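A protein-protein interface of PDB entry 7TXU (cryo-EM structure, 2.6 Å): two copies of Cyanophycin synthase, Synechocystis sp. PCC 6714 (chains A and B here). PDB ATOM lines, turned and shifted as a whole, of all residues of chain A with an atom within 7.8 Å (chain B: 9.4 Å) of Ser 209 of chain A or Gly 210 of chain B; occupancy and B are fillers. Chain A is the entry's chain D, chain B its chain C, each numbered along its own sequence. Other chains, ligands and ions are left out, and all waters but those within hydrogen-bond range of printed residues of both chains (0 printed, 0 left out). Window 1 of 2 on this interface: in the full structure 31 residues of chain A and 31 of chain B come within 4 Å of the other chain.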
ATOM      1  N   ARG A 200      37.662 -12.080 -22.245  1.00  0.00           N
ATOM      2  CA  ARG A 200      37.333 -11.058 -21.261  1.00  0.00           C
ATOM      3  C   ARG A 200      36.748 -11.651 -20.008  1.00  0.00           C
ATOM      4  O   ARG A 200      36.057 -12.674 -20.055  1.00  0.00           O
ATOM      5  CB  ARG A 200      36.321 -10.071 -21.791  1.00  0.00           C
ATOM      6  CG  ARG A 200      36.752  -9.259 -22.931  1.00  0.00           C
ATOM      7  CD  ARG A 200      35.701  -8.377 -23.365  1.00  0.00           C
ATOM      8  NE  ARG A 200      36.080  -7.654 -24.544  1.00  0.00           N
ATOM      9  CZ  ARG A 200      35.268  -6.872 -25.278  1.00  0.00           C
ATOM     10  NH1 ARG A 200      34.020  -6.717 -24.943  1.00  0.00           N
ATOM     11  NH2 ARG A 200      35.735  -6.263 -26.338  1.00  0.00           N
ATOM     12  N   THR A 204      33.841 -12.836 -11.551  1.00  0.00           N
ATOM     13  CA  THR A 204      33.656 -14.271 -11.715  1.00  0.00           C
ATOM     14  C   THR A 204      32.811 -14.701 -12.919  1.00  0.00           C
ATOM     15  O   THR A 204      32.435 -15.865 -13.024  1.00  0.00           O
ATOM     16  CB  THR A 204      33.149 -14.820 -10.382  1.00  0.00           C
ATOM     17  OG1 THR A 204      31.988 -14.044  -9.988  1.00  0.00           O
ATOM     18  CG2 THR A 204      34.246 -14.688  -9.367  1.00  0.00           C
ATOM     19  N   LEU A 205      32.482 -13.759 -13.800  1.00  0.00           N
ATOM     20  CA  LEU A 205      31.804 -14.028 -15.064  1.00  0.00           C
ATOM     21  C   LEU A 205      32.818 -13.935 -16.177  1.00  0.00           C
ATOM     22  O   LEU A 205      33.736 -13.121 -16.119  1.00  0.00           O
ATOM     23  CB  LEU A 205      30.664 -13.048 -15.369  1.00  0.00           C
ATOM     24  CG  LEU A 205      29.459 -13.022 -14.469  1.00  0.00           C
ATOM     25  CD1 LEU A 205      28.596 -11.899 -14.874  1.00  0.00           C
ATOM     26  CD2 LEU A 205      28.664 -14.329 -14.613  1.00  0.00           C
ATOM     27  N   SER A 206      32.641 -14.705 -17.230  1.00  0.00           N
ATOM     28  CA  SER A 206      33.586 -14.632 -18.336  1.00  0.00           C
ATOM     29  C   SER A 206      32.915 -14.651 -19.677  1.00  0.00           C
ATOM     30  O   SER A 206      31.703 -14.804 -19.804  1.00  0.00           O
ATOM     31  CB  SER A 206      34.552 -15.793 -18.296  1.00  0.00           C
ATOM     32  OG  SER A 206      33.929 -16.973 -18.675  1.00  0.00           O
ATOM     33  N   SER A 207      33.733 -14.565 -20.702  1.00  0.00           N
ATOM     34  CA  SER A 207      33.348 -14.624 -22.099  1.00  0.00           C
ATOM     35  C   SER A 207      32.686 -15.953 -22.490  1.00  0.00           C
ATOM     36  O   SER A 207      32.107 -16.058 -23.567  1.00  0.00           O
ATOM     37  CB  SER A 207      34.572 -14.372 -22.943  1.00  0.00           C
ATOM     38  OG  SER A 207      35.527 -15.350 -22.666  1.00  0.00           O
ATOM     39  N   HIS A 208      32.778 -16.980 -21.633  1.00  0.00           N
ATOM     40  CA  HIS A 208      32.133 -18.262 -21.881  1.00  0.00           C
ATOM     41  C   HIS A 208      30.846 -18.463 -21.072  1.00  0.00           C
ATOM     42  O   HIS A 208      30.234 -19.524 -21.155  1.00  0.00           O
ATOM     43  CB  HIS A 208      33.035 -19.446 -21.548  1.00  0.00           C
ATOM     44  CG  HIS A 208      34.231 -19.640 -22.400  1.00  0.00           C
ATOM     45  ND1 HIS A 208      35.011 -20.748 -22.291  1.00  0.00           N
ATOM     46  CD2 HIS A 208      34.790 -18.896 -23.369  1.00  0.00           C
ATOM     47  CE1 HIS A 208      35.994 -20.679 -23.145  1.00  0.00           C
ATOM     48  NE2 HIS A 208      35.880 -19.571 -23.812  1.00  0.00           N
ATOM     49  N   SER A 209      30.419 -17.462 -20.308  1.00  0.00           N
ATOM     50  CA  SER A 209      29.219 -17.598 -19.495  1.00  0.00           C
ATOM     51  C   SER A 209      28.010 -17.158 -20.300  1.00  0.00           C
ATOM     52  O   SER A 209      27.928 -16.011 -20.726  1.00  0.00           O
ATOM     53  CB  SER A 209      29.303 -16.742 -18.243  1.00  0.00           C
ATOM     54  OG  SER A 209      30.350 -17.142 -17.389  1.00  0.00           O
ATOM     55  N   GLY A 210      27.064 -18.059 -20.525  1.00  0.00           N
ATOM     56  CA  GLY A 210      25.905 -17.727 -21.334  1.00  0.00           C
ATOM     57  C   GLY A 210      24.846 -17.006 -20.549  1.00  0.00           C
ATOM     58  O   GLY A 210      24.674 -17.249 -19.361  1.00  0.00           O
ATOM     59  N   ILE A 211      24.058 -16.216 -21.240  1.00  0.00           N
ATOM     60  CA  ILE A 211      22.984 -15.482 -20.616  1.00  0.00           C
ATOM     61  C   ILE A 211      21.816 -16.335 -20.173  1.00  0.00           C
ATOM     62  O   ILE A 211      21.186 -16.025 -19.175  1.00  0.00           O
ATOM     63  CB  ILE A 211      22.516 -14.319 -21.513  1.00  0.00           C
ATOM     64  CG1 ILE A 211      21.659 -13.381 -20.665  1.00  0.00           C
ATOM     65  CG2 ILE A 211      21.787 -14.801 -22.754  1.00  0.00           C
ATOM     66  CD1 ILE A 211      21.379 -12.068 -21.255  1.00  0.00           C
ATOM     67  N   LEU A 212      21.489 -17.385 -20.902  1.00  0.00           N
ATOM     68  CA  LEU A 212      20.337 -18.157 -20.504  1.00  0.00           C
ATOM     69  C   LEU A 212      20.611 -18.908 -19.215  1.00  0.00           C
ATOM     70  O   LEU A 212      19.729 -19.003 -18.364  1.00  0.00           O
ATOM     71  CB  LEU A 212      19.944 -19.128 -21.611  1.00  0.00           C
ATOM     72  CG  LEU A 212      19.444 -18.508 -22.964  1.00  0.00           C
ATOM     73  CD1 LEU A 212      19.224 -19.608 -23.928  1.00  0.00           C
ATOM     74  CD2 LEU A 212      18.205 -17.709 -22.789  1.00  0.00           C
ATOM     75  N   GLY A 213      21.837 -19.416 -19.048  1.00  0.00           N
ATOM     76  CA  GLY A 213      22.232 -20.133 -17.842  1.00  0.00           C
ATOM     77  C   GLY A 213      22.251 -19.208 -16.647  1.00  0.00           C
ATOM     78  O   GLY A 213      21.769 -19.556 -15.572  1.00  0.00           O
ATOM     79  N   VAL A 214      22.787 -18.004 -16.837  1.00  0.00           N
ATOM     80  CA  VAL A 214      22.877 -17.033 -15.766  1.00  0.00           C
ATOM     81  C   VAL A 214      21.511 -16.557 -15.332  1.00  0.00           C
ATOM     82  O   VAL A 214      21.294 -16.372 -14.141  1.00  0.00           O
ATOM     83  CB  VAL A 214      23.788 -15.860 -16.156  1.00  0.00           C
ATOM     84  CG1 VAL A 214      23.731 -14.771 -15.123  1.00  0.00           C
ATOM     85  CG2 VAL A 214      25.212 -16.352 -16.275  1.00  0.00           C
ATOM     86  N   GLY A 424      23.287 -24.980 -17.081  1.00  0.00           N
ATOM     87  CA  GLY A 424      23.971 -24.338 -18.182  1.00  0.00           C
ATOM     88  C   GLY A 424      25.035 -23.335 -17.774  1.00  0.00           C
ATOM     89  O   GLY A 424      25.267 -22.364 -18.491  1.00  0.00           O
ATOM     90  N   LEU A 425      25.645 -23.513 -16.606  1.00  0.00           N
ATOM     91  CA  LEU A 425      26.686 -22.589 -16.148  1.00  0.00           C
ATOM     92  C   LEU A 425      28.084 -23.139 -16.333  1.00  0.00           C
ATOM     93  O   LEU A 425      28.291 -24.335 -16.177  1.00  0.00           O
ATOM     94  CB  LEU A 425      26.481 -22.287 -14.672  1.00  0.00           C
ATOM     95  CG  LEU A 425      25.190 -21.621 -14.256  1.00  0.00           C
ATOM     96  CD1 LEU A 425      25.142 -21.557 -12.779  1.00  0.00           C
ATOM     97  CD2 LEU A 425      25.118 -20.244 -14.788  1.00  0.00           C
ATOM     98  N   ASP A 426      29.071 -22.279 -16.645  1.00  0.00           N
ATOM     99  CA  ASP A 426      30.447 -22.759 -16.695  1.00  0.00           C
ATOM    100  C   ASP A 426      31.022 -22.739 -15.287  1.00  0.00           C
ATOM    101  O   ASP A 426      31.299 -23.785 -14.716  1.00  0.00           O
ATOM    102  CB  ASP A 426      31.289 -21.961 -17.678  1.00  0.00           C
ATOM    103  CG  ASP A 426      31.277 -20.506 -17.447  1.00  0.00           C
ATOM    104  OD1 ASP A 426      30.335 -20.005 -16.811  1.00  0.00           O
ATOM    105  OD2 ASP A 426      32.232 -19.879 -17.803  1.00  0.00           O
ATOM    106  N   ILE A 427      31.027 -21.581 -14.659  1.00  0.00           N
ATOM    107  CA  ILE A 427      31.504 -21.500 -13.291  1.00  0.00           C
ATOM    108  C   ILE A 427      30.298 -21.393 -12.391  1.00  0.00           C
ATOM    109  O   ILE A 427      29.516 -20.455 -12.505  1.00  0.00           O
ATOM    110  CB  ILE A 427      32.433 -20.299 -13.055  1.00  0.00           C
ATOM    111  CG1 ILE A 427      33.619 -20.397 -13.983  1.00  0.00           C
ATOM    112  CG2 ILE A 427      32.904 -20.307 -11.590  1.00  0.00           C
ATOM    113  CD1 ILE A 427      34.469 -19.167 -14.060  1.00  0.00           C
ATOM    114  N   ALA A 453      25.338 -18.306 -10.029  1.00  0.00           N
ATOM    115  CA  ALA A 453      26.187 -17.853 -11.102  1.00  0.00           C
ATOM    116  C   ALA A 453      27.178 -16.896 -10.478  1.00  0.00           C
ATOM    117  O   ALA A 453      26.850 -16.229  -9.505  1.00  0.00           O
ATOM    118  CB  ALA A 453      25.388 -17.185 -12.196  1.00  0.00           C
ATOM    119  N   ALA A 454      28.371 -16.811 -11.029  1.00  0.00           N
ATOM    120  CA  ALA A 454      29.402 -15.892 -10.557  1.00  0.00           C
ATOM    121  C   ALA A 454      29.716 -15.958  -9.052  1.00  0.00           C
ATOM    122  O   ALA A 454      29.895 -14.901  -8.457  1.00  0.00           O
ATOM    123  CB  ALA A 454      28.969 -14.476 -10.865  1.00  0.00           C
ATOM    124  N   MET A 478      40.289 -23.232 -19.078  1.00  0.00           N
ATOM    125  CA  MET A 478      39.205 -23.366 -20.032  1.00  0.00           C
ATOM    126  C   MET A 478      39.274 -22.220 -21.018  1.00  0.00           C
ATOM    127  O   MET A 478      38.942 -22.383 -22.188  1.00  0.00           O
ATOM    128  CB  MET A 478      37.821 -23.438 -19.385  1.00  0.00           C
ATOM    129  CG  MET A 478      37.266 -22.162 -18.895  1.00  0.00           C
ATOM    130  SD  MET A 478      35.688 -22.296 -18.172  1.00  0.00           S
ATOM    131  CE  MET A 478      35.574 -20.621 -17.650  1.00  0.00           C
ATOM    132  N   LEU A 479      39.747 -21.060 -20.558  1.00  0.00           N
ATOM    133  CA  LEU A 479      39.820 -19.899 -21.425  1.00  0.00           C
ATOM    134  C   LEU A 479      40.944 -20.017 -22.432  1.00  0.00           C
ATOM    135  O   LEU A 479      40.779 -19.663 -23.596  1.00  0.00           O
ATOM    136  CB  LEU A 479      40.013 -18.639 -20.596  1.00  0.00           C
ATOM    137  CG  LEU A 479      38.868 -18.206 -19.673  1.00  0.00           C
ATOM    138  CD1 LEU A 479      39.335 -17.036 -18.880  1.00  0.00           C
ATOM    139  CD2 LEU A 479      37.617 -17.859 -20.454  1.00  0.00           C
ATOM    140  N   LEU B 205      17.886 -14.768 -28.721  1.00  0.00           N
ATOM    141  CA  LEU B 205      19.070 -15.047 -27.913  1.00  0.00           C
ATOM    142  C   LEU B 205      19.339 -16.531 -27.960  1.00  0.00           C
ATOM    143  O   LEU B 205      18.411 -17.332 -28.009  1.00  0.00           O
ATOM    144  CB  LEU B 205      18.921 -14.633 -26.444  1.00  0.00           C
ATOM    145  CG  LEU B 205      18.758 -13.174 -26.107  1.00  0.00           C
ATOM    146  CD1 LEU B 205      18.475 -13.058 -24.666  1.00  0.00           C
ATOM    147  CD2 LEU B 205      20.054 -12.411 -26.417  1.00  0.00           C
ATOM    148  N   SER B 206      20.593 -16.925 -27.880  1.00  0.00           N
ATOM    149  CA  SER B 206      20.895 -18.350 -27.902  1.00  0.00           C
ATOM    150  C   SER B 206      21.943 -18.738 -26.901  1.00  0.00           C
ATOM    151  O   SER B 206      22.531 -17.911 -26.211  1.00  0.00           O
ATOM    152  CB  SER B 206      21.392 -18.773 -29.264  1.00  0.00           C
ATOM    153  OG  SER B 206      22.683 -18.316 -29.488  1.00  0.00           O
ATOM    154  N   SER B 207      22.227 -20.021 -26.874  1.00  0.00           N
ATOM    155  CA  SER B 207      23.243 -20.644 -26.046  1.00  0.00           C
ATOM    156  C   SER B 207      24.662 -20.133 -26.340  1.00  0.00           C
ATOM    157  O   SER B 207      25.583 -20.396 -25.569  1.00  0.00           O
ATOM    158  CB  SER B 207      23.165 -22.137 -26.237  1.00  0.00           C
ATOM    159  OG  SER B 207      23.390 -22.437 -27.582  1.00  0.00           O
ATOM    160  N   HIS B 208      24.857 -19.418 -27.455  1.00  0.00           N
ATOM    161  CA  HIS B 208      26.150 -18.836 -27.792  1.00  0.00           C
ATOM    162  C   HIS B 208      26.231 -17.332 -27.512  1.00  0.00           C
ATOM    163  O   HIS B 208      27.254 -16.713 -27.800  1.00  0.00           O
ATOM    164  CB  HIS B 208      26.509 -19.018 -29.264  1.00  0.00           C
ATOM    165  CG  HIS B 208      26.767 -20.400 -29.728  1.00  0.00           C
ATOM    166  ND1 HIS B 208      27.246 -20.654 -30.974  1.00  0.00           N
ATOM    167  CD2 HIS B 208      26.629 -21.599 -29.139  1.00  0.00           C
ATOM    168  CE1 HIS B 208      27.387 -21.941 -31.135  1.00  0.00           C
ATOM    169  NE2 HIS B 208      27.026 -22.534 -30.039  1.00  0.00           N
ATOM    170  N   SER B 209      25.187 -16.736 -26.946  1.00  0.00           N
ATOM    171  CA  SER B 209      25.191 -15.306 -26.678  1.00  0.00           C
ATOM    172  C   SER B 209      25.758 -15.052 -25.293  1.00  0.00           C
ATOM    173  O   SER B 209      25.213 -15.518 -24.300  1.00  0.00           O
ATOM    174  CB  SER B 209      23.786 -14.731 -26.736  1.00  0.00           C
ATOM    175  OG  SER B 209      23.212 -14.845 -28.019  1.00  0.00           O
ATOM    176  N   GLY B 210      26.860 -14.320 -25.209  1.00  0.00           N
ATOM    177  CA  GLY B 210      27.492 -14.081 -23.924  1.00  0.00           C
ATOM    178  C   GLY B 210      26.846 -12.957 -23.168  1.00  0.00           C
ATOM    179  O   GLY B 210      26.362 -12.001 -23.763  1.00  0.00           O
ATOM    180  N   ILE B 211      26.953 -13.007 -21.861  1.00  0.00           N
ATOM    181  CA  ILE B 211      26.400 -11.979 -21.015  1.00  0.00           C
ATOM    182  C   ILE B 211      27.136 -10.659 -21.067  1.00  0.00           C
ATOM    183  O   ILE B 211      26.515  -9.616 -20.937  1.00  0.00           O
ATOM    184  CB  ILE B 211      26.253 -12.478 -19.563  1.00  0.00           C
ATOM    185  CG1 ILE B 211      25.344 -11.504 -18.816  1.00  0.00           C
ATOM    186  CG2 ILE B 211      27.594 -12.657 -18.875  1.00  0.00           C
ATOM    187  CD1 ILE B 211      24.843 -11.970 -17.519  1.00  0.00           C
ATOM    188  N   LEU B 212      28.446 -10.673 -21.227  1.00  0.00           N
ATOM    189  CA  LEU B 212      29.145  -9.410 -21.217  1.00  0.00           C
ATOM    190  C   LEU B 212      28.819  -8.604 -22.458  1.00  0.00           C
ATOM    191  O   LEU B 212      28.665  -7.386 -22.374  1.00  0.00           O
ATOM    192  CB  LEU B 212      30.648  -9.642 -21.112  1.00  0.00           C
ATOM    193  CG  LEU B 212      31.183 -10.300 -19.791  1.00  0.00           C
ATOM    194  CD1 LEU B 212      32.635 -10.533 -19.940  1.00  0.00           C
ATOM    195  CD2 LEU B 212      30.907  -9.459 -18.597  1.00  0.00           C
ATOM    196  N   GLY B 213      28.682  -9.274 -23.608  1.00  0.00           N
ATOM    197  CA  GLY B 213      28.341  -8.616 -24.864  1.00  0.00           C
ATOM    198  C   GLY B 213      26.942  -8.046 -24.811  1.00  0.00           C
ATOM    199  O   GLY B 213      26.703  -6.919 -25.236  1.00  0.00           O
ATOM    200  N   VAL B 214      26.006  -8.819 -24.262  1.00  0.00           N
ATOM    201  CA  VAL B 214      24.626  -8.391 -24.166  1.00  0.00           C
ATOM    202  C   VAL B 214      24.470  -7.220 -23.225  1.00  0.00           C
ATOM    203  O   VAL B 214      23.688  -6.323 -23.512  1.00  0.00           O
ATOM    204  CB  VAL B 214      23.710  -9.560 -23.771  1.00  0.00           C
ATOM    205  CG1 VAL B 214      22.316  -9.077 -23.492  1.00  0.00           C
ATOM    206  CG2 VAL B 214      23.668 -10.563 -24.901  1.00  0.00           C
ATOM    207  N   GLU B 215      25.133  -7.239 -22.068  1.00  0.00           N
ATOM    208  CA  GLU B 215      25.041  -6.108 -21.163  1.00  0.00           C
ATOM    209  C   GLU B 215      25.726  -4.862 -21.703  1.00  0.00           C
ATOM    210  O   GLU B 215      25.189  -3.772 -21.571  1.00  0.00           O
ATOM    211  CB  GLU B 215      25.576  -6.457 -19.800  1.00  0.00           C
ATOM    212  CG  GLU B 215      24.703  -7.408 -19.040  1.00  0.00           C
ATOM    213  CD  GLU B 215      25.238  -7.719 -17.691  1.00  0.00           C
ATOM    214  OE1 GLU B 215      26.394  -7.468 -17.461  1.00  0.00           O
ATOM    215  OE2 GLU B 215      24.484  -8.187 -16.865  1.00  0.00           O
ATOM    216  N   LEU B 216      26.864  -4.993 -22.381  1.00  0.00           N
ATOM    217  CA  LEU B 216      27.535  -3.828 -22.941  1.00  0.00           C
ATOM    218  C   LEU B 216      26.678  -3.163 -23.990  1.00  0.00           C
ATOM    219  O   LEU B 216      26.551  -1.949 -24.001  1.00  0.00           O
ATOM    220  CB  LEU B 216      28.886  -4.221 -23.553  1.00  0.00           C
ATOM    221  CG  LEU B 216      29.741  -3.107 -24.228  1.00  0.00           C
ATOM    222  CD1 LEU B 216      30.098  -2.005 -23.260  1.00  0.00           C
ATOM    223  CD2 LEU B 216      30.981  -3.738 -24.791  1.00  0.00           C
ATOM    224  N   ALA B 217      26.007  -3.949 -24.817  1.00  0.00           N
ATOM    225  CA  ALA B 217      25.151  -3.454 -25.881  1.00  0.00           C
ATOM    226  C   ALA B 217      23.932  -2.694 -25.362  1.00  0.00           C
ATOM    227  O   ALA B 217      23.242  -2.033 -26.143  1.00  0.00           O
ATOM    228  CB  ALA B 217      24.685  -4.608 -26.737  1.00  0.00           C
ATOM    229  N   CYS B 218      23.589  -2.845 -24.085  1.00  0.00           N
ATOM    230  CA  CYS B 218      22.419  -2.200 -23.529  1.00  0.00           C
ATOM    231  C   CYS B 218      22.784  -0.922 -22.791  1.00  0.00           C
ATOM    232  O   CYS B 218      21.918  -0.207 -22.286  1.00  0.00           O
ATOM    233  CB  CYS B 218      21.717  -3.148 -22.585  1.00  0.00           C
ATOM    234  SG  CYS B 218      21.104  -4.632 -23.398  1.00  0.00           S
ATOM    235  N   ILE B 423      32.014  -5.313 -29.866  1.00  0.00           N
ATOM    236  CA  ILE B 423      31.065  -5.392 -28.764  1.00  0.00           C
ATOM    237  C   ILE B 423      31.017  -6.805 -28.182  1.00  0.00           C
ATOM    238  O   ILE B 423      30.925  -6.965 -26.971  1.00  0.00           O
ATOM    239  CB  ILE B 423      29.659  -4.902 -29.167  1.00  0.00           C
ATOM    240  CG1 ILE B 423      29.709  -3.397 -29.606  1.00  0.00           C
ATOM    241  CG2 ILE B 423      28.634  -5.106 -28.019  1.00  0.00           C
ATOM    242  CD1 ILE B 423      30.231  -2.396 -28.592  1.00  0.00           C
ATOM    243  N   GLY B 424      31.043  -7.838 -29.020  1.00  0.00           N
ATOM    244  CA  GLY B 424      31.017  -9.193 -28.513  1.00  0.00           C
ATOM    245  C   GLY B 424      29.692  -9.912 -28.686  1.00  0.00           C
ATOM    246  O   GLY B 424      29.345 -10.759 -27.865  1.00  0.00           O
ATOM    247  N   LEU B 425      28.914  -9.551 -29.701  1.00  0.00           N
ATOM    248  CA  LEU B 425      27.621 -10.204 -29.932  1.00  0.00           C
ATOM    249  C   LEU B 425      27.669 -11.220 -31.053  1.00  0.00           C
ATOM    250  O   LEU B 425      28.372 -11.010 -32.032  1.00  0.00           O
ATOM    251  CB  LEU B 425      26.579  -9.155 -30.280  1.00  0.00           C
ATOM    252  CG  LEU B 425      26.271  -8.091 -29.254  1.00  0.00           C
ATOM    253  CD1 LEU B 425      25.348  -7.103 -29.853  1.00  0.00           C
ATOM    254  CD2 LEU B 425      25.619  -8.683 -28.066  1.00  0.00           C
ATOM    255  N   ASP B 426      26.908 -12.325 -30.946  1.00  0.00           N
ATOM    256  CA  ASP B 426      26.830 -13.251 -32.070  1.00  0.00           C
ATOM    257  C   ASP B 426      25.776 -12.750 -33.043  1.00  0.00           C
ATOM    258  O   ASP B 426      26.096 -12.352 -34.155  1.00  0.00           O
ATOM    259  CB  ASP B 426      26.568 -14.677 -31.610  1.00  0.00           C
ATOM    260  CG  ASP B 426      25.378 -14.830 -30.756  1.00  0.00           C
ATOM    261  OD1 ASP B 426      24.943 -13.840 -30.146  1.00  0.00           O
ATOM    262  OD2 ASP B 426      24.823 -15.890 -30.761  1.00  0.00           O
ATOM    263  N   ILE B 427      24.554 -12.592 -32.572  1.00  0.00           N
ATOM    264  CA  ILE B 427      23.510 -12.059 -33.429  1.00  0.00           C
ATOM    265  C   ILE B 427      23.289 -10.619 -33.037  1.00  0.00           C
ATOM    266  O   ILE B 427      22.936 -10.330 -31.899  1.00  0.00           O
ATOM    267  CB  ILE B 427      22.191 -12.837 -33.311  1.00  0.00           C
ATOM    268  CG1 ILE B 427      22.430 -14.282 -33.670  1.00  0.00           C
ATOM    269  CG2 ILE B 427      21.155 -12.217 -34.265  1.00  0.00           C
ATOM    270  CD1 ILE B 427      21.304 -15.214 -33.345  1.00  0.00           C
ATOM    271  N   ALA B 453      21.265  -6.144 -29.090  1.00  0.00           N
ATOM    272  CA  ALA B 453      21.305  -7.559 -28.820  1.00  0.00           C
ATOM    273  C   ALA B 453      19.906  -8.075 -29.076  1.00  0.00           C
ATOM    274  O   ALA B 453      18.942  -7.344 -28.882  1.00  0.00           O
ATOM    275  CB  ALA B 453      21.745  -7.840 -27.403  1.00  0.00           C
ATOM    276  N   ALA B 454      19.782  -9.318 -29.491  1.00  0.00           N
ATOM    277  CA  ALA B 454      18.491  -9.954 -29.727  1.00  0.00           C
ATOM    278  C   ALA B 454      17.524  -9.183 -30.641  1.00  0.00           C
ATOM    279  O   ALA B 454      16.340  -9.150 -30.328  1.00  0.00           O
ATOM    280  CB  ALA B 454      17.795 -10.146 -28.398  1.00  0.00           C
ATOM    281  N   MET B 478      25.356 -21.841 -37.249  1.00  0.00           N
ATOM    282  CA  MET B 478      26.389 -21.652 -36.249  1.00  0.00           C
ATOM    283  C   MET B 478      26.132 -22.594 -35.093  1.00  0.00           C
ATOM    284  O   MET B 478      27.068 -23.083 -34.467  1.00  0.00           O
ATOM    285  CB  MET B 478      26.509 -20.209 -35.752  1.00  0.00           C
ATOM    286  CG  MET B 478      25.472 -19.761 -34.804  1.00  0.00           C
ATOM    287  SD  MET B 478      25.654 -18.115 -34.265  1.00  0.00           S
ATOM    288  CE  MET B 478      24.163 -18.052 -33.336  1.00  0.00           C
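The backbone carbonyl oxygen of Ser 209 of chain B is in hydrogen-bond range of the backbone NH of Ile 211 of chain A (3.3 Å).
The backbone carbonyl oxygen (O) of Ser 209 of chain A is in hydrogen-bond range of the backbone NH (N) of Ile 211 of chain B (3.4 Å).
The side-chain hydroxyl of Ser 209 of chain B sits at hydrogen-bond distance from the backbone NH of Ser 206 of chain B, 3.3 Å away.
OG of Ser 209 of chain B sits at hydrogen-bond distance from OD1 of Asp 426 of chain B (2.9 Å).
The backbone carbonyl oxygen (O) of Val 214 of chain B lies within hydrogen-bond range of the side-chain sulfur (SG) of Cys 218 of chain B.
N of Ser 207 of chain A is in hydrogen-bond range of O of Arg 200 of chain A, at 3.1 Å.
N of Ser 206 of chain A lies within hydrogen-bond range of OG of Ser 209 of chain A.
OG of Ser 209 of chain A lies within hydrogen-bond range of OD1 of Asp 426 of chain A, at 2.9 Å.
Arg 200 of chain A touches Ile 423 of chain B.
CA of Gly 210 of chain B touches O of Ser 209 of chain A, 3.8 Å away.
Gly 210 of chain A touches Ser 209 of chain B.
Ile 211 of chain A touches Val 214 of chain B.
Ile 211 of chain B touches Val 214 of chain A (CD1 to CG1, 3.9 Å).
Ser 209 of chain A touches just these residues of chain B: Gly 210 and Ile 211.
Of chain A, only Ser 209 (3.8 Å) comes within 4 Å of Gly 210 of chain B.
No residue of chain B comes within 4 Å of Ser 206 of chain A.
Of the printed residues of chain A, Ile 211 of chain B touches Ser 209 and Val 214.
Of the printed residues of chain B, Val 214 of chain A touches Ile 211.
Of the printed residues of chain B, Ile 211 of chain A touches Ser 209 (3.3 Å) and Val 214 (3.9 Å).
Printed residues of chain A within 4 Å of Ile 423 of chain B: Arg 200.
Printed residues of chain B within 4 Å of Arg 200 of chain A: Ile 423 (3.7 Å).
The nearest residue of chain B that does not touch Ser 209 of chain A is Ser 209 of chain B (4.5 Å).
Of the 20 printed residues of chain A, 5 touch a printed residue of chain B.
Among the printed residues, 7 pairs touch across the chains.
Among the printed residues, no Asp or Glu carboxylate lies within 4 Å of a Lys or Arg side-chain nitrogen of the other chain.
Ser 209 of chain A touches Gly 210 of chain B, and with the chains exchanged Gly 210 of chain A touches Ser 209 of chain B.
Ser 209 of chain A touches Ile 211 of chain B, and with the chains exchanged Ile 211 of chain A touches Ser 209 of chain B.
Ile 211 of chain A touches Val 214 of chain B, and with the chains exchanged Val 214 of chain A touches Ile 211 of chain B.
Positions printed for both chains: 205, 206, 207, 208, 209, 210, 211, 212, 213, 214, 424, 425, 426, 427, 453, 454 and 478.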
